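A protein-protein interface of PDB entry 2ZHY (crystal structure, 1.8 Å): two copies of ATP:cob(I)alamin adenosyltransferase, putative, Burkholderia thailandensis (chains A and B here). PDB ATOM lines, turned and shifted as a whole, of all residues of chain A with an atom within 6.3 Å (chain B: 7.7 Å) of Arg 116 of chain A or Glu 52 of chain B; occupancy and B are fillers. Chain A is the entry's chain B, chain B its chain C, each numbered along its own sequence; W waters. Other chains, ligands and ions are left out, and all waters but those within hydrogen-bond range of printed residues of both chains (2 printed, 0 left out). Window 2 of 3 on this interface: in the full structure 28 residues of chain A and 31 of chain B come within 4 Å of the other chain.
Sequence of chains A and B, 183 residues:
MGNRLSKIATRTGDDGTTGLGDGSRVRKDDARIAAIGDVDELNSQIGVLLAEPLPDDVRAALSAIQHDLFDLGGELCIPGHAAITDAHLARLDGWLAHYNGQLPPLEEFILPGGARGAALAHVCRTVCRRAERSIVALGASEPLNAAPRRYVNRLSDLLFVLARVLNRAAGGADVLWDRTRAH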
ATOM      1  N   LEU A  49      19.685  12.348  16.122  1.00  0.00           N
ATOM      2  CA  LEU A  49      20.543  12.668  14.986  1.00  0.00           C
ATOM      3  C   LEU A  49      21.186  14.047  15.218  1.00  0.00           C
ATOM      4  O   LEU A  49      22.362  14.257  14.905  1.00  0.00           O
ATOM      5  CB  LEU A  49      19.718  12.712  13.694  1.00  0.00           C
ATOM      6  CG  LEU A  49      20.369  12.341  12.350  1.00  0.00           C
ATOM      7  CD1 LEU A  49      19.728  13.187  11.261  1.00  0.00           C
ATOM      8  CD2 LEU A  49      21.878  12.549  12.369  1.00  0.00           C
ATOM      9  N   GLU A  52      24.417  14.593  17.083  1.00  0.00           N
ATOM     10  CA  GLU A  52      25.638  14.191  16.390  1.00  0.00           C
ATOM     11  C   GLU A  52      26.313  15.407  15.765  1.00  0.00           C
ATOM     12  O   GLU A  52      25.714  16.482  15.679  1.00  0.00           O
ATOM     13  CB  GLU A  52      25.317  13.200  15.263  1.00  0.00           C
ATOM     14  CG  GLU A  52      24.844  11.824  15.709  1.00  0.00           C
ATOM     15  CD  GLU A  52      25.936  11.024  16.394  1.00  0.00           C
ATOM     16  OE1 GLU A  52      27.000  10.816  15.772  1.00  0.00           O
ATOM     17  OE2 GLU A  52      25.729  10.601  17.551  1.00  0.00           O
ATOM     18  N   GLY A 114      26.518   3.425   7.008  1.00  0.00           N
ATOM     19  CA  GLY A 114      27.659   4.238   6.639  1.00  0.00           C
ATOM     20  C   GLY A 114      28.123   4.965   7.878  1.00  0.00           C
ATOM     21  O   GLY A 114      28.228   4.362   8.944  1.00  0.00           O
ATOM     22  N   ALA A 115      28.401   6.258   7.751  1.00  0.00           N
ATOM     23  CA  ALA A 115      28.820   7.049   8.897  1.00  0.00           C
ATOM     24  C   ALA A 115      27.673   7.030   9.910  1.00  0.00           C
ATOM     25  O   ALA A 115      26.509   6.946   9.525  1.00  0.00           O
ATOM     26  CB  ALA A 115      29.116   8.470   8.461  1.00  0.00           C
ATOM     27  N   ARG A 116      28.005   7.103  11.196  1.00  0.00           N
ATOM     28  CA  ARG A 116      26.993   7.083  12.250  1.00  0.00           C
ATOM     29  C   ARG A 116      25.840   8.052  11.987  1.00  0.00           C
ATOM     30  O   ARG A 116      24.668   7.686  12.118  1.00  0.00           O
ATOM     31  CB  ARG A 116      27.632   7.400  13.602  1.00  0.00           C
ATOM     32  CG  ARG A 116      26.645   7.407  14.761  1.00  0.00           C
ATOM     33  CD  ARG A 116      27.387   7.484  16.079  1.00  0.00           C
ATOM     34  NE  ARG A 116      28.185   6.282  16.303  1.00  0.00           N
ATOM     35  CZ  ARG A 116      29.354   6.261  16.936  1.00  0.00           C
ATOM     36  NH1 ARG A 116      29.879   7.385  17.411  1.00  0.00           N
ATOM     37  NH2 ARG A 116      30.001   5.114  17.094  1.00  0.00           N
ATOM     38  N   GLY A 117      26.173   9.285  11.627  1.00  0.00           N
ATOM     39  CA  GLY A 117      25.143  10.267  11.344  1.00  0.00           C
ATOM     40  C   GLY A 117      24.261   9.829  10.186  1.00  0.00           C
ATOM     41  O   GLY A 117      23.045  10.026  10.214  1.00  0.00           O
ATOM     42  N   ALA A 118      24.868   9.234   9.164  1.00  0.00           N
ATOM     43  CA  ALA A 118      24.107   8.771   8.005  1.00  0.00           C
ATOM     44  C   ALA A 118      23.189   7.616   8.399  1.00  0.00           C
ATOM     45  O   ALA A 118      22.032   7.566   7.978  1.00  0.00           O
ATOM     46  CB  ALA A 118      25.046   8.328   6.892  1.00  0.00           C
ATOM     47  N   ALA A 119      23.704   6.687   9.200  1.00  0.00           N
ATOM     48  CA  ALA A 119      22.905   5.545   9.638  1.00  0.00           C
ATOM     49  C   ALA A 119      21.686   6.012  10.445  1.00  0.00           C
ATOM     50  O   ALA A 119      20.577   5.513  10.248  1.00  0.00           O
ATOM     51  CB  ALA A 119      23.753   4.603  10.474  1.00  0.00           C
ATOM     52  N   LEU A 120      21.897   6.966  11.350  1.00  0.00           N
ATOM     53  CA  LEU A 120      20.809   7.495  12.166  1.00  0.00           C
ATOM     54  C   LEU A 120      19.764   8.189  11.295  1.00  0.00           C
ATOM     55  O   LEU A 120      18.570   8.137  11.587  1.00  0.00           O
ATOM     56  CB  LEU A 120      21.351   8.472  13.218  1.00  0.00           C
ATOM     57  CG  LEU A 120      22.122   7.806  14.369  1.00  0.00           C
ATOM     58  CD1 LEU A 120      22.855   8.859  15.199  1.00  0.00           C
ATOM     59  CD2 LEU A 120      21.148   7.023  15.241  1.00  0.00           C
ATOM     60  N   ALA A 121      20.208   8.828  10.218  1.00  0.00           N
ATOM     61  CA  ALA A 121      19.275   9.509   9.324  1.00  0.00           C
ATOM     62  C   ALA A 121      18.375   8.467   8.645  1.00  0.00           C
ATOM     63  O   ALA A 121      17.187   8.705   8.418  1.00  0.00           O
ATOM     64  CB  ALA A 121      20.042  10.322   8.285  1.00  0.00           C
ATOM     65  N   ASN A 167      27.083  11.012   4.575  1.00  0.00           N
ATOM     66  CA  ASN A 167      28.119  10.047   4.226  1.00  0.00           C
ATOM     67  C   ASN A 167      29.179  10.752   3.381  1.00  0.00           C
ATOM     68  O   ASN A 167      30.363  10.428   3.446  1.00  0.00           O
ATOM     69  CB  ASN A 167      27.540   8.862   3.444  1.00  0.00           C
ATOM     70  CG  ASN A 167      27.171   7.699   4.343  1.00  0.00           C
ATOM     71  OD1 ASN A 167      27.884   7.395   5.296  1.00  0.00           O
ATOM     72  ND2 ASN A 167      26.064   7.033   4.036  1.00  0.00           N
ATOM     73  N   ILE B  46      20.383  -1.937  12.037  1.00  0.00           N
ATOM     74  CA  ILE B  46      21.592  -2.747  11.941  1.00  0.00           C
ATOM     75  C   ILE B  46      22.690  -1.846  11.376  1.00  0.00           C
ATOM     76  O   ILE B  46      23.857  -1.977  11.740  1.00  0.00           O
ATOM     77  CB  ILE B  46      21.372  -3.983  11.045  1.00  0.00           C
ATOM     78  CG1 ILE B  46      20.495  -4.994  11.794  1.00  0.00           C
ATOM     79  CG2 ILE B  46      22.713  -4.594  10.645  1.00  0.00           C
ATOM     80  CD1 ILE B  46      20.165  -6.248  10.998  1.00  0.00           C
ATOM     81  N   GLY B  47      22.292  -0.910  10.518  1.00  0.00           N
ATOM     82  CA  GLY B  47      23.234   0.035   9.941  1.00  0.00           C
ATOM     83  C   GLY B  47      23.854   0.883  11.038  1.00  0.00           C
ATOM     84  O   GLY B  47      25.045   1.196  11.000  1.00  0.00           O
ATOM     85  N   VAL B  48      23.043   1.264  12.024  1.00  0.00           N
ATOM     86  CA  VAL B  48      23.550   2.048  13.143  1.00  0.00           C
ATOM     87  C   VAL B  48      24.546   1.182  13.906  1.00  0.00           C
ATOM     88  O   VAL B  48      25.615   1.648  14.294  1.00  0.00           O
ATOM     89  CB  VAL B  48      22.410   2.498  14.090  1.00  0.00           C
ATOM     90  CG1 VAL B  48      22.996   3.090  15.372  1.00  0.00           C
ATOM     91  CG2 VAL B  48      21.541   3.538  13.389  1.00  0.00           C
ATOM     92  N   LEU B  49      24.190  -0.083  14.117  1.00  0.00           N
ATOM     93  CA  LEU B  49      25.075  -1.019  14.808  1.00  0.00           C
ATOM     94  C   LEU B  49      26.407  -1.171  14.061  1.00  0.00           C
ATOM     95  O   LEU B  49      27.468  -1.259  14.676  1.00  0.00           O
ATOM     96  CB  LEU B  49      24.394  -2.387  14.952  1.00  0.00           C
ATOM     97  CG  LEU B  49      25.205  -3.538  15.560  1.00  0.00           C
ATOM     98  CD1 LEU B  49      25.886  -3.085  16.840  1.00  0.00           C
ATOM     99  CD2 LEU B  49      24.275  -4.718  15.826  1.00  0.00           C
ATOM    100  N   LEU B  50      26.349  -1.193  12.732  1.00  0.00           N
ATOM    101  CA  LEU B  50      27.555  -1.325  11.918  1.00  0.00           C
ATOM    102  C   LEU B  50      28.450  -0.085  11.989  1.00  0.00           C
ATOM    103  O   LEU B  50      29.582  -0.119  11.513  1.00  0.00           O
ATOM    104  CB  LEU B  50      27.180  -1.617  10.459  1.00  0.00           C
ATOM    105  CG  LEU B  50      26.736  -3.059  10.173  1.00  0.00           C
ATOM    106  CD1 LEU B  50      26.018  -3.132   8.839  1.00  0.00           C
ATOM    107  CD2 LEU B  50      27.956  -3.977  10.175  1.00  0.00           C
ATOM    108  N   ALA B  51      27.954   1.000  12.585  1.00  0.00           N
ATOM    109  CA  ALA B  51      28.750   2.227  12.713  1.00  0.00           C
ATOM    110  C   ALA B  51      29.560   2.204  14.004  1.00  0.00           C
ATOM    111  O   ALA B  51      30.289   3.151  14.313  1.00  0.00           O
ATOM    112  CB  ALA B  51      27.846   3.465  12.679  1.00  0.00           C
ATOM    113  N   GLU B  52      29.411   1.117  14.757  1.00  0.00           N
ATOM    114  CA  GLU B  52      30.130   0.915  16.009  1.00  0.00           C
ATOM    115  C   GLU B  52      31.380   0.095  15.722  1.00  0.00           C
ATOM    116  O   GLU B  52      31.512  -0.493  14.650  1.00  0.00           O
ATOM    117  CB  GLU B  52      29.270   0.106  16.988  1.00  0.00           C
ATOM    118  CG  GLU B  52      28.024   0.807  17.485  1.00  0.00           C
ATOM    119  CD  GLU B  52      28.354   1.961  18.411  1.00  0.00           C
ATOM    120  OE1 GLU B  52      28.995   1.719  19.458  1.00  0.00           O
ATOM    121  OE2 GLU B  52      27.981   3.105  18.088  1.00  0.00           O
ATOM    122  N   PRO B  53      32.333   0.075  16.664  1.00  0.00           N
ATOM    123  CA  PRO B  53      33.536  -0.729  16.433  1.00  0.00           C
ATOM    124  C   PRO B  53      33.039  -2.160  16.638  1.00  0.00           C
ATOM    125  O   PRO B  53      32.275  -2.411  17.568  1.00  0.00           O
ATOM    126  CB  PRO B  53      34.481  -0.272  17.544  1.00  0.00           C
ATOM    127  CG  PRO B  53      33.540   0.184  18.635  1.00  0.00           C
ATOM    128  CD  PRO B  53      32.481   0.923  17.860  1.00  0.00           C
ATOM    129  N   LEU B  54      33.455  -3.087  15.782  1.00  0.00           N
ATOM    130  CA  LEU B  54      32.994  -4.471  15.880  1.00  0.00           C
ATOM    131  C   LEU B  54      34.079  -5.487  15.576  1.00  0.00           C
ATOM    132  O   LEU B  54      35.069  -5.178  14.909  1.00  0.00           O
ATOM    133  CB  LEU B  54      31.869  -4.725  14.872  1.00  0.00           C
ATOM    134  CG  LEU B  54      30.567  -3.920  14.882  1.00  0.00           C
ATOM    135  CD1 LEU B  54      29.794  -4.203  13.588  1.00  0.00           C
ATOM    136  CD2 LEU B  54      29.740  -4.297  16.104  1.00  0.00           C
ATOM    137  N   PRO B  55      33.908  -6.720  16.075  1.00  0.00           N
ATOM    138  CA  PRO B  55      34.905  -7.751  15.793  1.00  0.00           C
ATOM    139  C   PRO B  55      34.711  -8.018  14.297  1.00  0.00           C
ATOM    140  O   PRO B  55      33.610  -7.820  13.770  1.00  0.00           O
ATOM    141  CB  PRO B  55      34.445  -8.925  16.655  1.00  0.00           C
ATOM    142  CG  PRO B  55      33.758  -8.260  17.806  1.00  0.00           C
ATOM    143  CD  PRO B  55      32.975  -7.163  17.127  1.00  0.00           C
ATOM    144  N   ARG B  59      31.029  -8.144  12.058  1.00  0.00           N
ATOM    145  CA  ARG B  59      30.765  -7.177  11.004  1.00  0.00           C
ATOM    146  C   ARG B  59      30.449  -7.842   9.670  1.00  0.00           C
ATOM    147  O   ARG B  59      29.569  -7.390   8.933  1.00  0.00           O
ATOM    148  CB  ARG B  59      31.957  -6.238  10.836  1.00  0.00           C
ATOM    149  CG  ARG B  59      31.780  -5.222   9.716  1.00  0.00           C
ATOM    150  CD  ARG B  59      32.958  -4.274   9.656  1.00  0.00           C
ATOM    151  NE  ARG B  59      33.032  -3.436  10.847  1.00  0.00           N
ATOM    152  CZ  ARG B  59      32.171  -2.464  11.126  1.00  0.00           C
ATOM    153  NH1 ARG B  59      31.165  -2.203  10.300  1.00  0.00           N
ATOM    154  NH2 ARG B  59      32.319  -1.747  12.229  1.00  0.00           N
ATOM    155  N   ALA B 115      27.690  -2.722  26.727  1.00  0.00           N
ATOM    156  CA  ALA B 115      28.449  -1.805  25.884  1.00  0.00           C
ATOM    157  C   ALA B 115      27.442  -1.256  24.865  1.00  0.00           C
ATOM    158  O   ALA B 115      26.424  -1.897  24.603  1.00  0.00           O
ATOM    159  CB  ALA B 115      29.570  -2.552  25.178  1.00  0.00           C
ATOM    160  N   ARG B 116      27.709  -0.085  24.297  1.00  0.00           N
ATOM    161  CA  ARG B 116      26.781   0.499  23.331  1.00  0.00           C
ATOM    162  C   ARG B 116      26.446  -0.463  22.191  1.00  0.00           C
ATOM    163  O   ARG B 116      25.288  -0.563  21.775  1.00  0.00           O
ATOM    164  CB  ARG B 116      27.344   1.809  22.766  1.00  0.00           C
ATOM    165  CG  ARG B 116      26.445   2.468  21.714  1.00  0.00           C
ATOM    166  CD  ARG B 116      26.828   3.931  21.465  1.00  0.00           C
ATOM    167  NE  ARG B 116      26.345   4.431  20.178  1.00  0.00           N
ATOM    168  CZ  ARG B 116      25.065   4.471  19.807  1.00  0.00           C
ATOM    169  NH1 ARG B 116      24.726   4.950  18.610  1.00  0.00           N
ATOM    170  NH2 ARG B 116      24.118   4.037  20.628  1.00  0.00           N
ATOM    171  N   GLY B 117      27.462  -1.172  21.697  1.00  0.00           N
ATOM    172  CA  GLY B 117      27.257  -2.126  20.618  1.00  0.00           C
ATOM    173  C   GLY B 117      26.300  -3.238  21.010  1.00  0.00           C
ATOM    174  O   GLY B 117      25.415  -3.609  20.238  1.00  0.00           O
ATOM    175  N   ALA B 118      26.472  -3.782  22.209  1.00  0.00           N
ATOM    176  CA  ALA B 118      25.590  -4.842  22.677  1.00  0.00           C
ATOM    177  C   ALA B 118      24.169  -4.289  22.866  1.00  0.00           C
ATOM    178  O   ALA B 118      23.182  -4.937  22.493  1.00  0.00           O
ATOM    179  CB  ALA B 118      26.112  -5.420  23.994  1.00  0.00           C
ATOM    180  N   LEU B 120      22.763  -1.804  21.307  1.00  0.00           N
ATOM    181  CA  LEU B 120      22.165  -1.571  19.997  1.00  0.00           C
ATOM    182  C   LEU B 120      21.740  -2.897  19.371  1.00  0.00           C
ATOM    183  O   LEU B 120      20.735  -2.965  18.664  1.00  0.00           O
ATOM    184  CB  LEU B 120      23.153  -0.838  19.082  1.00  0.00           C
ATOM    185  CG  LEU B 120      23.450   0.630  19.435  1.00  0.00           C
ATOM    186  CD1 LEU B 120      24.591   1.159  18.563  1.00  0.00           C
ATOM    187  CD2 LEU B 120      22.193   1.469  19.238  1.00  0.00           C
ATOM    188  N   ALA B 121      22.501  -3.955  19.641  1.00  0.00           N
ATOM    189  CA  ALA B 121      22.174  -5.272  19.108  1.00  0.00           C
ATOM    190  C   ALA B 121      20.819  -5.717  19.655  1.00  0.00           C
ATOM    191  O   ALA B 121      20.044  -6.365  18.955  1.00  0.00           O
ATOM    192  CB  ALA B 121      23.258  -6.288  19.487  1.00  0.00           C
ATOM    193  N   LEU B 166      29.268  -9.119  21.586  1.00  0.00           N
ATOM    194  CA  LEU B 166      29.726  -7.733  21.578  1.00  0.00           C
ATOM    195  C   LEU B 166      30.152  -7.209  22.952  1.00  0.00           C
ATOM    196  O   LEU B 166      31.092  -6.416  23.056  1.00  0.00           O
ATOM    197  CB  LEU B 166      28.649  -6.833  20.971  1.00  0.00           C
ATOM    198  CG  LEU B 166      28.383  -7.098  19.484  1.00  0.00           C
ATOM    199  CD1 LEU B 166      27.354  -6.114  18.957  1.00  0.00           C
ATOM    200  CD2 LEU B 166      29.684  -6.967  18.700  1.00  0.00           C
HETATM  201  O   HOH W   1      26.616   1.432   8.799  1.00  0.00           O
HETATM  202  O   HOH W   2      26.311   3.722  16.067  1.00  0.00           O
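Water W1 bridges the backbone NH (N) of Gly 114 of chain A and the backbone carbonyl oxygen (O) of Gly 47 of chain B.
Water W2 lies within hydrogen-bond range of OE2 of Glu 52 of chain B (2.7 Å), O of Val 48 of chain B (2.8 Å), NE of Arg 116 of chain A (3.2 Å) and NH1 of Arg 116 of chain B (3.2 Å).
OE2 of Glu 52 of chain B is in salt-bridge range of NE of Arg 116 of chain B, at 3.0 Å.
O of Glu 52 of chain B lies within hydrogen-bond range of NH2 of Arg 59 of chain B (2.8 Å).
NH2 of Arg 116 of chain A sits at hydrogen-bond distance from O of Ala 51 of chain B (3.4 Å).
The guanidinium group (NH2) of Arg 116 of chain A is in salt-bridge range of the side-chain carboxylate (OE2) of Glu 52 of chain B, 3.0 Å away.
Printed residues of chain A that touch a printed residue of chain B: Gly 114, Arg 116, Ala 119 and Leu 120.
Hydrophobic or aromatic side chains of chain A that line the printed part of chain B: Ala 119 and Leu 120.
Of the 18 printed residues of chain B, 4 touch a printed residue of chain A.
Among the printed residues, 6 pairs touch across the chains.
Among the printed residues, Asp or Glu carboxylates within 4 Å of a Lys or Arg side-chain nitrogen of the other chain: Arg 116 of chain A with Glu 52 of chain B (3.0 Å).
Arg 116 of chain A touches Glu 52 of chain B, but with the chains exchanged Glu 52 of chain A does not touch Arg 116 of chain B (5.8 Å).
Of the 6 pairs that touch across the chains among the printed residues, none has its exchanged pair printed and touching as well.
Of the printed residues of chain B, Gly 114 of chain A touches Ala 51.
No residue of chain B comes within 4 Å of Ala 115 of chain A.
Printed residues of chain B within 4 Å of Arg 116 of chain A: Ala 51 (3.4 Å) and Glu 52 (3.0 Å).
Printed residues of chain B within 4 Å of Ala 119 of chain A: Gly 47 and Val 48.
Of the printed residues of chain B, Leu 120 of chain A touches Val 48 (3.97 Å).
Ala 121 of chain A touches none of the printed residues of chain B.
Printed residues of chain A within 4 Å of Val 48 of chain B: Ala 119 (3.7 Å) and Leu 120 (3.97 Å).
Printed residues of chain A within 4 Å of Ala 51 of chain B: Gly 114 (3.9 Å) and Arg 116 (3.4 Å).
The nearest printed residue of chain A that does not touch Glu 52 of chain B is Gly 114 of chain A (6.8 Å).
Ala 51 of chain B touches Gly 114 of chain A (CB to O, 3.9 Å).
Ala 119 of chain A touches Gly 47 of chain B (CB to O, 3.7 Å).
CB of Ala 119 of chain A touches CA of Val 48 of chain B, at 3.7 Å.
Val 48 of chain B touches Leu 120 of chain A.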
